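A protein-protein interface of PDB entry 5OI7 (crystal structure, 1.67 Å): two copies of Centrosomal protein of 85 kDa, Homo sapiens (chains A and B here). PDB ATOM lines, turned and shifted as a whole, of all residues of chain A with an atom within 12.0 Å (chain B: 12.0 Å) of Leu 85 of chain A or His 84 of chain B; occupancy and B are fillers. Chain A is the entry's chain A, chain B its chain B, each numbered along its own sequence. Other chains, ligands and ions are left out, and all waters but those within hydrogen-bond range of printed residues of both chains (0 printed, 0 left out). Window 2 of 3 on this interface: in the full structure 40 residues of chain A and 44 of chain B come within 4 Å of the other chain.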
ATOM      1  N   GLU A  76       9.161  -0.296  20.504  1.00  0.00           N
ATOM      2  CA  GLU A  76       8.411   0.515  21.458  1.00  0.00           C
ATOM      3  C   GLU A  76       9.150   0.636  22.785  1.00  0.00           C
ATOM      4  O   GLU A  76       9.175   1.713  23.392  1.00  0.00           O
ATOM      5  CB  GLU A  76       7.016  -0.073  21.670  1.00  0.00           C
ATOM      6  CG  GLU A  76       6.311   0.489  22.896  1.00  0.00           C
ATOM      7  CD  GLU A  76       4.842   0.129  22.948  1.00  0.00           C
ATOM      8  OE1 GLU A  76       4.096   0.540  22.036  1.00  0.00           O
ATOM      9  OE2 GLU A  76       4.436  -0.571  23.899  1.00  0.00           O
ATOM     10  N   LYS A  77       9.756  -0.456  23.256  1.00  0.00           N
ATOM     11  CA  LYS A  77      10.489  -0.394  24.519  1.00  0.00           C
ATOM     12  C   LYS A  77      11.709   0.510  24.403  1.00  0.00           C
ATOM     13  O   LYS A  77      12.069   1.208  25.360  1.00  0.00           O
ATOM     14  CB  LYS A  77      10.888  -1.801  24.965  1.00  0.00           C
ATOM     15  CG  LYS A  77       9.692  -2.707  25.228  1.00  0.00           C
ATOM     16  CD  LYS A  77      10.059  -3.925  26.062  1.00  0.00           C
ATOM     17  CE  LYS A  77      10.792  -4.974  25.246  1.00  0.00           C
ATOM     18  NZ  LYS A  77      10.977  -6.234  26.025  1.00  0.00           N
ATOM     19  N   ASN A  78      12.353   0.524  23.236  1.00  0.00           N
ATOM     20  CA  ASN A  78      13.485   1.424  23.048  1.00  0.00           C
ATOM     21  C   ASN A  78      13.038   2.879  23.088  1.00  0.00           C
ATOM     22  O   ASN A  78      13.695   3.720  23.717  1.00  0.00           O
ATOM     23  CB  ASN A  78      14.197   1.103  21.735  1.00  0.00           C
ATOM     24  CG  ASN A  78      15.013  -0.175  21.819  1.00  0.00           C
ATOM     25  OD1 ASN A  78      15.259  -0.697  22.908  1.00  0.00           O
ATOM     26  ND2 ASN A  78      15.445  -0.681  20.669  1.00  0.00           N
ATOM     27  N   LEU A  79      11.916   3.195  22.439  1.00  0.00           N
ATOM     28  CA  LEU A  79      11.396   4.557  22.495  1.00  0.00           C
ATOM     29  C   LEU A  79      11.079   4.961  23.928  1.00  0.00           C
ATOM     30  O   LEU A  79      11.298   6.114  24.320  1.00  0.00           O
ATOM     31  CB  LEU A  79      10.159   4.680  21.608  1.00  0.00           C
ATOM     32  CG  LEU A  79      10.434   4.514  20.113  1.00  0.00           C
ATOM     33  CD1 LEU A  79       9.161   4.713  19.305  1.00  0.00           C
ATOM     34  CD2 LEU A  79      11.521   5.483  19.665  1.00  0.00           C
ATOM     35  N   THR A  80      10.576   4.020  24.732  1.00  0.00           N
ATOM     36  CA  THR A  80      10.292   4.325  26.132  1.00  0.00           C
ATOM     37  C   THR A  80      11.564   4.694  26.885  1.00  0.00           C
ATOM     38  O   THR A  80      11.582   5.673  27.641  1.00  0.00           O
ATOM     39  CB  THR A  80       9.594   3.141  26.797  1.00  0.00           C
ATOM     40  OG1 THR A  80       8.329   2.936  26.159  1.00  0.00           O
ATOM     41  CG2 THR A  80       9.371   3.411  28.279  1.00  0.00           C
ATOM     42  N   LEU A  81      12.641   3.932  26.687  1.00  0.00           N
ATOM     43  CA  LEU A  81      13.898   4.270  27.345  1.00  0.00           C
ATOM     44  C   LEU A  81      14.422   5.619  26.868  1.00  0.00           C
ATOM     45  O   LEU A  81      14.947   6.404  27.665  1.00  0.00           O
ATOM     46  CB  LEU A  81      14.934   3.174  27.108  1.00  0.00           C
ATOM     47  CG  LEU A  81      14.600   1.814  27.728  1.00  0.00           C
ATOM     48  CD1 LEU A  81      15.725   0.823  27.489  1.00  0.00           C
ATOM     49  CD2 LEU A  81      14.310   1.951  29.214  1.00  0.00           C
ATOM     50  N   GLN A  82      14.288   5.910  25.570  1.00  0.00           N
ATOM     51  CA  GLN A  82      14.755   7.197  25.065  1.00  0.00           C
ATOM     52  C   GLN A  82      13.972   8.349  25.679  1.00  0.00           C
ATOM     53  O   GLN A  82      14.538   9.410  25.965  1.00  0.00           O
ATOM     54  CB  GLN A  82      14.652   7.235  23.543  1.00  0.00           C
ATOM     55  CG  GLN A  82      15.610   6.303  22.837  1.00  0.00           C
ATOM     56  CD  GLN A  82      15.500   6.415  21.334  1.00  0.00           C
ATOM     57  OE1 GLN A  82      14.696   5.726  20.708  1.00  0.00           O
ATOM     58  NE2 GLN A  82      16.301   7.295  20.745  1.00  0.00           N
ATOM     59  N   GLU A  83      12.664   8.166  25.878  1.00  0.00           N
ATOM     60  CA  GLU A  83      11.872   9.217  26.508  1.00  0.00           C
ATOM     61  C   GLU A  83      12.312   9.442  27.949  1.00  0.00           C
ATOM     62  O   GLU A  83      12.398  10.588  28.406  1.00  0.00           O
ATOM     63  CB  GLU A  83      10.384   8.871  26.440  1.00  0.00           C
ATOM     64  CG  GLU A  83       9.773   9.063  25.058  1.00  0.00           C
ATOM     65  CD  GLU A  83       9.694  10.529  24.647  1.00  0.00           C
ATOM     66  OE1 GLU A  83       9.348  11.371  25.502  1.00  0.00           O
ATOM     67  OE2 GLU A  83       9.979  10.837  23.469  1.00  0.00           O
ATOM     68  N   HIS A  84      12.614   8.359  28.672  1.00  0.00           N
ATOM     69  CA  HIS A  84      13.090   8.483  30.047  1.00  0.00           C
ATOM     70  C   HIS A  84      14.440   9.185  30.124  1.00  0.00           C
ATOM     71  O   HIS A  84      14.771   9.774  31.161  1.00  0.00           O
ATOM     72  CB  HIS A  84      13.189   7.102  30.697  1.00  0.00           C
ATOM     73  CG  HIS A  84      11.893   6.594  31.246  1.00  0.00           C
ATOM     74  ND1 HIS A  84      11.384   5.353  30.927  1.00  0.00           N
ATOM     75  CD2 HIS A  84      11.009   7.153  32.107  1.00  0.00           C
ATOM     76  CE1 HIS A  84      10.238   5.174  31.559  1.00  0.00           C
ATOM     77  NE2 HIS A  84       9.987   6.251  32.281  1.00  0.00           N
ATOM     78  N   LEU A  85      15.239   9.117  29.062  1.00  0.00           N
ATOM     79  CA  LEU A  85      16.548   9.755  29.065  1.00  0.00           C
ATOM     80  C   LEU A  85      16.504  11.210  28.624  1.00  0.00           C
ATOM     81  O   LEU A  85      17.535  11.889  28.687  1.00  0.00           O
ATOM     82  CB  LEU A  85      17.520   8.985  28.167  1.00  0.00           C
ATOM     83  CG  LEU A  85      18.019   7.654  28.725  1.00  0.00           C
ATOM     84  CD1 LEU A  85      18.602   6.799  27.609  1.00  0.00           C
ATOM     85  CD2 LEU A  85      19.054   7.896  29.815  1.00  0.00           C
ATOM     86  N   ARG A  86      15.348  11.698  28.184  1.00  0.00           N
ATOM     87  CA  ARG A  86      15.243  13.079  27.734  1.00  0.00           C
ATOM     88  C   ARG A  86      15.600  14.047  28.851  1.00  0.00           C
ATOM     89  O   ARG A  86      15.257  13.835  30.017  1.00  0.00           O
ATOM     90  CB  ARG A  86      13.829  13.379  27.238  1.00  0.00           C
ATOM     91  CG  ARG A  86      13.492  12.771  25.888  1.00  0.00           C
ATOM     92  CD  ARG A  86      12.047  13.059  25.526  1.00  0.00           C
ATOM     93  NE  ARG A  86      11.789  14.492  25.419  1.00  0.00           N
ATOM     94  CZ  ARG A  86      10.600  15.019  25.150  1.00  0.00           C
ATOM     95  NH1 ARG A  86       9.550  14.230  24.963  1.00  0.00           N
ATOM     96  NH2 ARG A  86      10.461  16.336  25.070  1.00  0.00           N
ATOM     97  N   GLN A  87      16.302  15.111  28.479  1.00  0.00           N
ATOM     98  CA  GLN A  87      16.550  16.238  29.362  1.00  0.00           C
ATOM     99  C   GLN A  87      15.798  17.487  28.920  1.00  0.00           C
ATOM    100  O   GLN A  87      15.786  18.480  29.655  1.00  0.00           O
ATOM    101  CB  GLN A  87      18.061  16.509  29.448  1.00  0.00           C
ATOM    102  CG  GLN A  87      18.814  15.354  30.113  1.00  0.00           C
ATOM    103  CD  GLN A  87      20.326  15.456  30.011  1.00  0.00           C
ATOM    104  OE1 GLN A  87      20.865  16.251  29.239  1.00  0.00           O
ATOM    105  NE2 GLN A  87      21.021  14.638  30.796  1.00  0.00           N
ATOM    106  N   ALA A  88      15.186  17.461  27.743  1.00  0.00           N
ATOM    107  CA  ALA A  88      14.320  18.529  27.269  1.00  0.00           C
ATOM    108  C   ALA A  88      13.373  17.935  26.235  1.00  0.00           C
ATOM    109  O   ALA A  88      13.507  16.761  25.882  1.00  0.00           O
ATOM    110  CB  ALA A  88      15.127  19.674  26.672  1.00  0.00           C
ATOM    111  N   LEU B  74      17.946  -4.620  17.735  1.00  0.00           N
ATOM    112  CA  LEU B  74      17.102  -3.919  18.697  1.00  0.00           C
ATOM    113  C   LEU B  74      17.453  -4.302  20.129  1.00  0.00           C
ATOM    114  O   LEU B  74      17.372  -3.466  21.039  1.00  0.00           O
ATOM    115  CB  LEU B  74      15.632  -4.215  18.409  1.00  0.00           C
ATOM    116  CG  LEU B  74      15.091  -3.639  17.103  1.00  0.00           C
ATOM    117  CD1 LEU B  74      13.751  -4.273  16.751  1.00  0.00           C
ATOM    118  CD2 LEU B  74      14.958  -2.128  17.209  1.00  0.00           C
ATOM    119  N   ILE B  75      17.834  -5.559  20.356  1.00  0.00           N
ATOM    120  CA  ILE B  75      18.254  -5.969  21.695  1.00  0.00           C
ATOM    121  C   ILE B  75      19.535  -5.250  22.097  1.00  0.00           C
ATOM    122  O   ILE B  75      19.671  -4.774  23.234  1.00  0.00           O
ATOM    123  CB  ILE B  75      18.426  -7.496  21.761  1.00  0.00           C
ATOM    124  CG1 ILE B  75      17.074  -8.192  21.632  1.00  0.00           C
ATOM    125  CG2 ILE B  75      19.116  -7.902  23.061  1.00  0.00           C
ATOM    126  CD1 ILE B  75      16.122  -7.873  22.758  1.00  0.00           C
ATOM    127  N   GLU B  76      20.495  -5.159  21.177  1.00  0.00           N
ATOM    128  CA  GLU B  76      21.739  -4.461  21.481  1.00  0.00           C
ATOM    129  C   GLU B  76      21.485  -2.981  21.743  1.00  0.00           C
ATOM    130  O   GLU B  76      22.057  -2.404  22.673  1.00  0.00           O
ATOM    131  CB  GLU B  76      22.739  -4.671  20.341  1.00  0.00           C
ATOM    132  CG  GLU B  76      23.185  -6.128  20.225  1.00  0.00           C
ATOM    133  CD  GLU B  76      24.040  -6.407  19.001  1.00  0.00           C
ATOM    134  OE1 GLU B  76      24.059  -5.573  18.074  1.00  0.00           O
ATOM    135  OE2 GLU B  76      24.699  -7.467  18.970  1.00  0.00           O
ATOM    136  N   LYS B  77      20.613  -2.356  20.947  1.00  0.00           N
ATOM    137  CA  LYS B  77      20.269  -0.956  21.179  1.00  0.00           C
ATOM    138  C   LYS B  77      19.594  -0.767  22.533  1.00  0.00           C
ATOM    139  O   LYS B  77      19.847   0.225  23.230  1.00  0.00           O
ATOM    140  CB  LYS B  77      19.365  -0.449  20.054  1.00  0.00           C
ATOM    141  CG  LYS B  77      20.069  -0.294  18.719  1.00  0.00           C
ATOM    142  CD  LYS B  77      19.097   0.120  17.621  1.00  0.00           C
ATOM    143  CE  LYS B  77      19.813   0.287  16.289  1.00  0.00           C
ATOM    144  NZ  LYS B  77      18.856   0.451  15.156  1.00  0.00           N
ATOM    145  N   ASN B  78      18.721  -1.703  22.913  1.00  0.00           N
ATOM    146  CA  ASN B  78      18.037  -1.621  24.201  1.00  0.00           C
ATOM    147  C   ASN B  78      19.028  -1.716  25.353  1.00  0.00           C
ATOM    148  O   ASN B  78      18.912  -0.988  26.349  1.00  0.00           O
ATOM    149  CB  ASN B  78      16.981  -2.727  24.286  1.00  0.00           C
ATOM    150  CG  ASN B  78      16.228  -2.736  25.606  1.00  0.00           C
ATOM    151  OD1 ASN B  78      16.684  -3.320  26.589  1.00  0.00           O
ATOM    152  ND2 ASN B  78      15.055  -2.116  25.622  1.00  0.00           N
ATOM    153  N   LEU B  79      20.023  -2.597  25.231  1.00  0.00           N
ATOM    154  CA  LEU B  79      21.056  -2.694  26.261  1.00  0.00           C
ATOM    155  C   LEU B  79      21.873  -1.410  26.345  1.00  0.00           C
ATOM    156  O   LEU B  79      22.224  -0.959  27.443  1.00  0.00           O
ATOM    157  CB  LEU B  79      21.965  -3.890  25.982  1.00  0.00           C
ATOM    158  CG  LEU B  79      21.340  -5.273  26.186  1.00  0.00           C
ATOM    159  CD1 LEU B  79      22.270  -6.369  25.689  1.00  0.00           C
ATOM    160  CD2 LEU B  79      20.998  -5.492  27.652  1.00  0.00           C
ATOM    161  N   THR B  80      22.198  -0.812  25.197  1.00  0.00           N
ATOM    162  CA  THR B  80      22.908   0.466  25.215  1.00  0.00           C
ATOM    163  C   THR B  80      22.095   1.531  25.939  1.00  0.00           C
ATOM    164  O   THR B  80      22.637   2.293  26.750  1.00  0.00           O
ATOM    165  CB  THR B  80      23.227   0.912  23.785  1.00  0.00           C
ATOM    166  OG1 THR B  80      24.125  -0.026  23.181  1.00  0.00           O
ATOM    167  CG2 THR B  80      23.869   2.297  23.779  1.00  0.00           C
ATOM    168  N   LEU B  81      20.790   1.599  25.659  1.00  0.00           N
ATOM    169  CA  LEU B  81      19.934   2.566  26.339  1.00  0.00           C
ATOM    170  C   LEU B  81      19.849   2.273  27.831  1.00  0.00           C
ATOM    171  O   LEU B  81      19.847   3.198  28.651  1.00  0.00           O
ATOM    172  CB  LEU B  81      18.545   2.566  25.708  1.00  0.00           C
ATOM    173  CG  LEU B  81      18.518   3.139  24.291  1.00  0.00           C
ATOM    174  CD1 LEU B  81      17.222   2.792  23.581  1.00  0.00           C
ATOM    175  CD2 LEU B  81      18.717   4.647  24.353  1.00  0.00           C
ATOM    176  N   GLN B  82      19.770   0.991  28.203  1.00  0.00           N
ATOM    177  CA  GLN B  82      19.760   0.639  29.619  1.00  0.00           C
ATOM    178  C   GLN B  82      21.023   1.128  30.315  1.00  0.00           C
ATOM    179  O   GLN B  82      20.970   1.578  31.465  1.00  0.00           O
ATOM    180  CB  GLN B  82      19.609  -0.874  29.792  1.00  0.00           C
ATOM    181  CG  GLN B  82      18.237  -1.411  29.435  1.00  0.00           C
ATOM    182  CD  GLN B  82      18.091  -2.883  29.765  1.00  0.00           C
ATOM    183  OE1 GLN B  82      18.457  -3.326  30.855  1.00  0.00           O
ATOM    184  NE2 GLN B  82      17.564  -3.653  28.821  1.00  0.00           N
ATOM    185  N   GLU B  83      22.170   1.053  29.637  1.00  0.00           N
ATOM    186  CA  GLU B  83      23.408   1.500  30.265  1.00  0.00           C
ATOM    187  C   GLU B  83      23.433   3.016  30.410  1.00  0.00           C
ATOM    188  O   GLU B  83      23.915   3.539  31.421  1.00  0.00           O
ATOM    189  CB  GLU B  83      24.617   1.011  29.470  1.00  0.00           C
ATOM    190  CG  GLU B  83      25.950   1.333  30.132  1.00  0.00           C
ATOM    191  CD  GLU B  83      26.045   0.803  31.558  1.00  0.00           C
ATOM    192  OE1 GLU B  83      25.478  -0.276  31.838  1.00  0.00           O
ATOM    193  OE2 GLU B  83      26.683   1.471  32.399  1.00  0.00           O
ATOM    194  N   HIS B  84      22.915   3.740  29.416  1.00  0.00           N
ATOM    195  CA  HIS B  84      22.786   5.186  29.567  1.00  0.00           C
ATOM    196  C   HIS B  84      21.917   5.532  30.767  1.00  0.00           C
ATOM    197  O   HIS B  84      22.179   6.516  31.467  1.00  0.00           O
ATOM    198  CB  HIS B  84      22.211   5.813  28.296  1.00  0.00           C
ATOM    199  CG  HIS B  84      23.221   6.001  27.206  1.00  0.00           C
ATOM    200  ND1 HIS B  84      24.313   6.832  27.340  1.00  0.00           N
ATOM    201  CD2 HIS B  84      23.300   5.475  25.961  1.00  0.00           C
ATOM    202  CE1 HIS B  84      25.025   6.803  26.227  1.00  0.00           C
ATOM    203  NE2 HIS B  84      24.432   5.987  25.375  1.00  0.00           N
ATOM    204  N   LEU B  85      20.877   4.734  31.022  1.00  0.00           N
ATOM    205  CA  LEU B  85      19.974   5.022  32.129  1.00  0.00           C
ATOM    206  C   LEU B  85      20.659   4.890  33.482  1.00  0.00           C
ATOM    207  O   LEU B  85      20.211   5.510  34.453  1.00  0.00           O
ATOM    208  CB  LEU B  85      18.760   4.091  32.064  1.00  0.00           C
ATOM    209  CG  LEU B  85      17.489   4.588  32.753  1.00  0.00           C
ATOM    210  CD1 LEU B  85      16.925   5.807  32.029  1.00  0.00           C
ATOM    211  CD2 LEU B  85      16.456   3.475  32.836  1.00  0.00           C
ATOM    212  N   ARG B  86      21.731   4.100  33.571  1.00  0.00           N
ATOM    213  CA  ARG B  86      22.474   4.002  34.821  1.00  0.00           C
ATOM    214  C   ARG B  86      23.290   5.254  35.115  1.00  0.00           C
ATOM    215  O   ARG B  86      23.782   5.400  36.241  1.00  0.00           O
ATOM    216  CB  ARG B  86      23.374   2.764  34.800  1.00  0.00           C
ATOM    217  CG  ARG B  86      22.573   1.469  34.850  1.00  0.00           C
ATOM    218  CD  ARG B  86      23.438   0.219  34.798  1.00  0.00           C
ATOM    219  NE  ARG B  86      22.611  -0.964  34.580  1.00  0.00           N
ATOM    220  CZ  ARG B  86      22.457  -1.561  33.402  1.00  0.00           C
ATOM    221  NH1 ARG B  86      23.099  -1.102  32.336  1.00  0.00           N
ATOM    222  NH2 ARG B  86      21.675  -2.627  33.292  1.00  0.00           N
ATOM    223  N   GLN B  87      23.438   6.162  34.150  1.00  0.00           N
ATOM    224  CA  GLN B  87      24.051   7.461  34.391  1.00  0.00           C
ATOM    225  C   GLN B  87      23.026   8.586  34.490  1.00  0.00           C
ATOM    226  O   GLN B  87      23.412   9.756  34.583  1.00  0.00           O
ATOM    227  CB  GLN B  87      25.076   7.781  33.297  1.00  0.00           C
ATOM    228  CG  GLN B  87      26.297   6.873  33.298  1.00  0.00           C
ATOM    229  CD  GLN B  87      26.085   5.609  32.493  1.00  0.00           C
ATOM    230  OE1 GLN B  87      25.702   5.664  31.324  1.00  0.00           O
ATOM    231  NE2 GLN B  87      26.332   4.459  33.115  1.00  0.00           N
ATOM    232  N   ALA B  88      21.736   8.262  34.480  1.00  0.00           N
ATOM    233  CA  ALA B  88      20.696   9.275  34.620  1.00  0.00           C
ATOM    234  C   ALA B  88      20.274   9.433  36.080  1.00  0.00           C
ATOM    235  O   ALA B  88      20.582   8.590  36.922  1.00  0.00           O
ATOM    236  CB  ALA B  88      19.492   8.925  33.756  1.00  0.00           C
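Of the printed residues of chain B, Leu 85 of chain A touches Leu 81, His 84 and Leu 85.
Of chain B, only Asn 78, Leu 81 and Gln 82 come within 4 Å of Leu 81 of chain A.
No residue of chain B comes within 4 Å of Glu 83 of chain A.
No residue of chain B comes within 4 Å of His 84 of chain A.
No residue of chain A comes within 4 Å of Thr 80 of chain B.
Of the printed residues of chain A, Leu 81 of chain B touches Asn 78 (3.6 Å), Leu 81 (3.8 Å), Gln 82 (3.8 Å) and Leu 85 (3.9 Å).
Of chain A, only Leu 85 (3.7 Å) comes within 4 Å of Leu 85 of chain B.
No residue of chain A comes within 4 Å of Gln 87 of chain B.
Of the printed residues of chain A, Gln 82 of chain B touches Leu 81.
Of the printed residues of chain B, Gln 82 of chain A touches Leu 81 (3.8 Å).
Of the printed residues of chain A, Leu 74 of chain B touches Asn 78 (3.4 Å).
Ala 88 of chain A touches none of the printed residues of chain B.
Thr 80 of chain A touches none of the printed residues of chain B.
The nearest printed residue of chain B that does not touch Leu 85 of chain A is Ala 88 of chain B (4.1 Å).
The nearest printed residue of chain A that does not touch Leu 74 of chain B is Glu 76 of chain A (6.9 Å).
ND2 of Asn 78 of chain A sits at hydrogen-bond distance from O of Leu 74 of chain B, at 3.4 Å.
OD1 of Asn 78 of chain A sits close to ND2 of Asn 78 of chain B (3.1 Å).
NE2 of Gln 82 of chain B sits at hydrogen-bond distance from OD1 of Asn 78 of chain B, 2.4 Å away.
Lys 77 of chain B touches Asn 78 of chain A.
O of Asn 78 of chain A touches CD1 of Leu 81 of chain B, 3.6 Å away.
CD1 of Leu 81 of chain A touches ND2 of Asn 78 of chain B, 3.5 Å away.
CD1 of Leu 81 of chain A touches CB of Leu 81 of chain B, at 3.8 Å.
CD1 of Leu 81 of chain A touches CG of Gln 82 of chain B (3.9 Å).
Gln 82 of chain A touches Leu 81 of chain B.
CD2 of Leu 81 of chain B touches CD1 of Leu 85 of chain A, at 3.9 Å.
Leu 85 of chain A touches His 84 of chain B (CD2 to O, 3.8 Å).
Leu 85 of chain B touches Leu 85 of chain A.
Printed residues of chain B that touch a printed residue of chain A: Leu 74, Lys 77, Asn 78, Leu 81, Gln 82, His 84 and Leu 85.
Hydrophobic or aromatic side chains of chain B within 4 Å of the printed part of chain A: Leu 74, Leu 81, His 84 and Leu 85.
Hydrophobic or aromatic side chains of chain A within 4 Å of the printed part of chain B: Leu 81 and Leu 85.
Along chain A the printed residues that touch a printed residue of chain B span positions 78 to 85.
Among the printed residues, 11 pairs touch across the chains.
Among the printed residues, no Asp or Glu carboxylate lies within 4 Å of a Lys or Arg side-chain nitrogen of the other chain.
Asn 78 of chain A touches Leu 81 of chain B, and with the chains exchanged Leu 81 of chain A touches Asn 78 of chain B.
Leu 81 of chain B touches its own counterpart, Leu 81 of chain A.
Leu 81 of chain A touches Gln 82 of chain B, and with the chains exchanged Gln 82 of chain A touches Leu 81 of chain B.
Leu 85 of chain B touches its own counterpart, Leu 85 of chain A.
Positions printed for both chains: 76, 77, 78, 79, 80, 81, 82, 83, 84, 85, 86, 87 and 88.
Of the 11 pairs that touch across the chains among the printed residues, 7 have their exchanged pair printed and touching as well.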
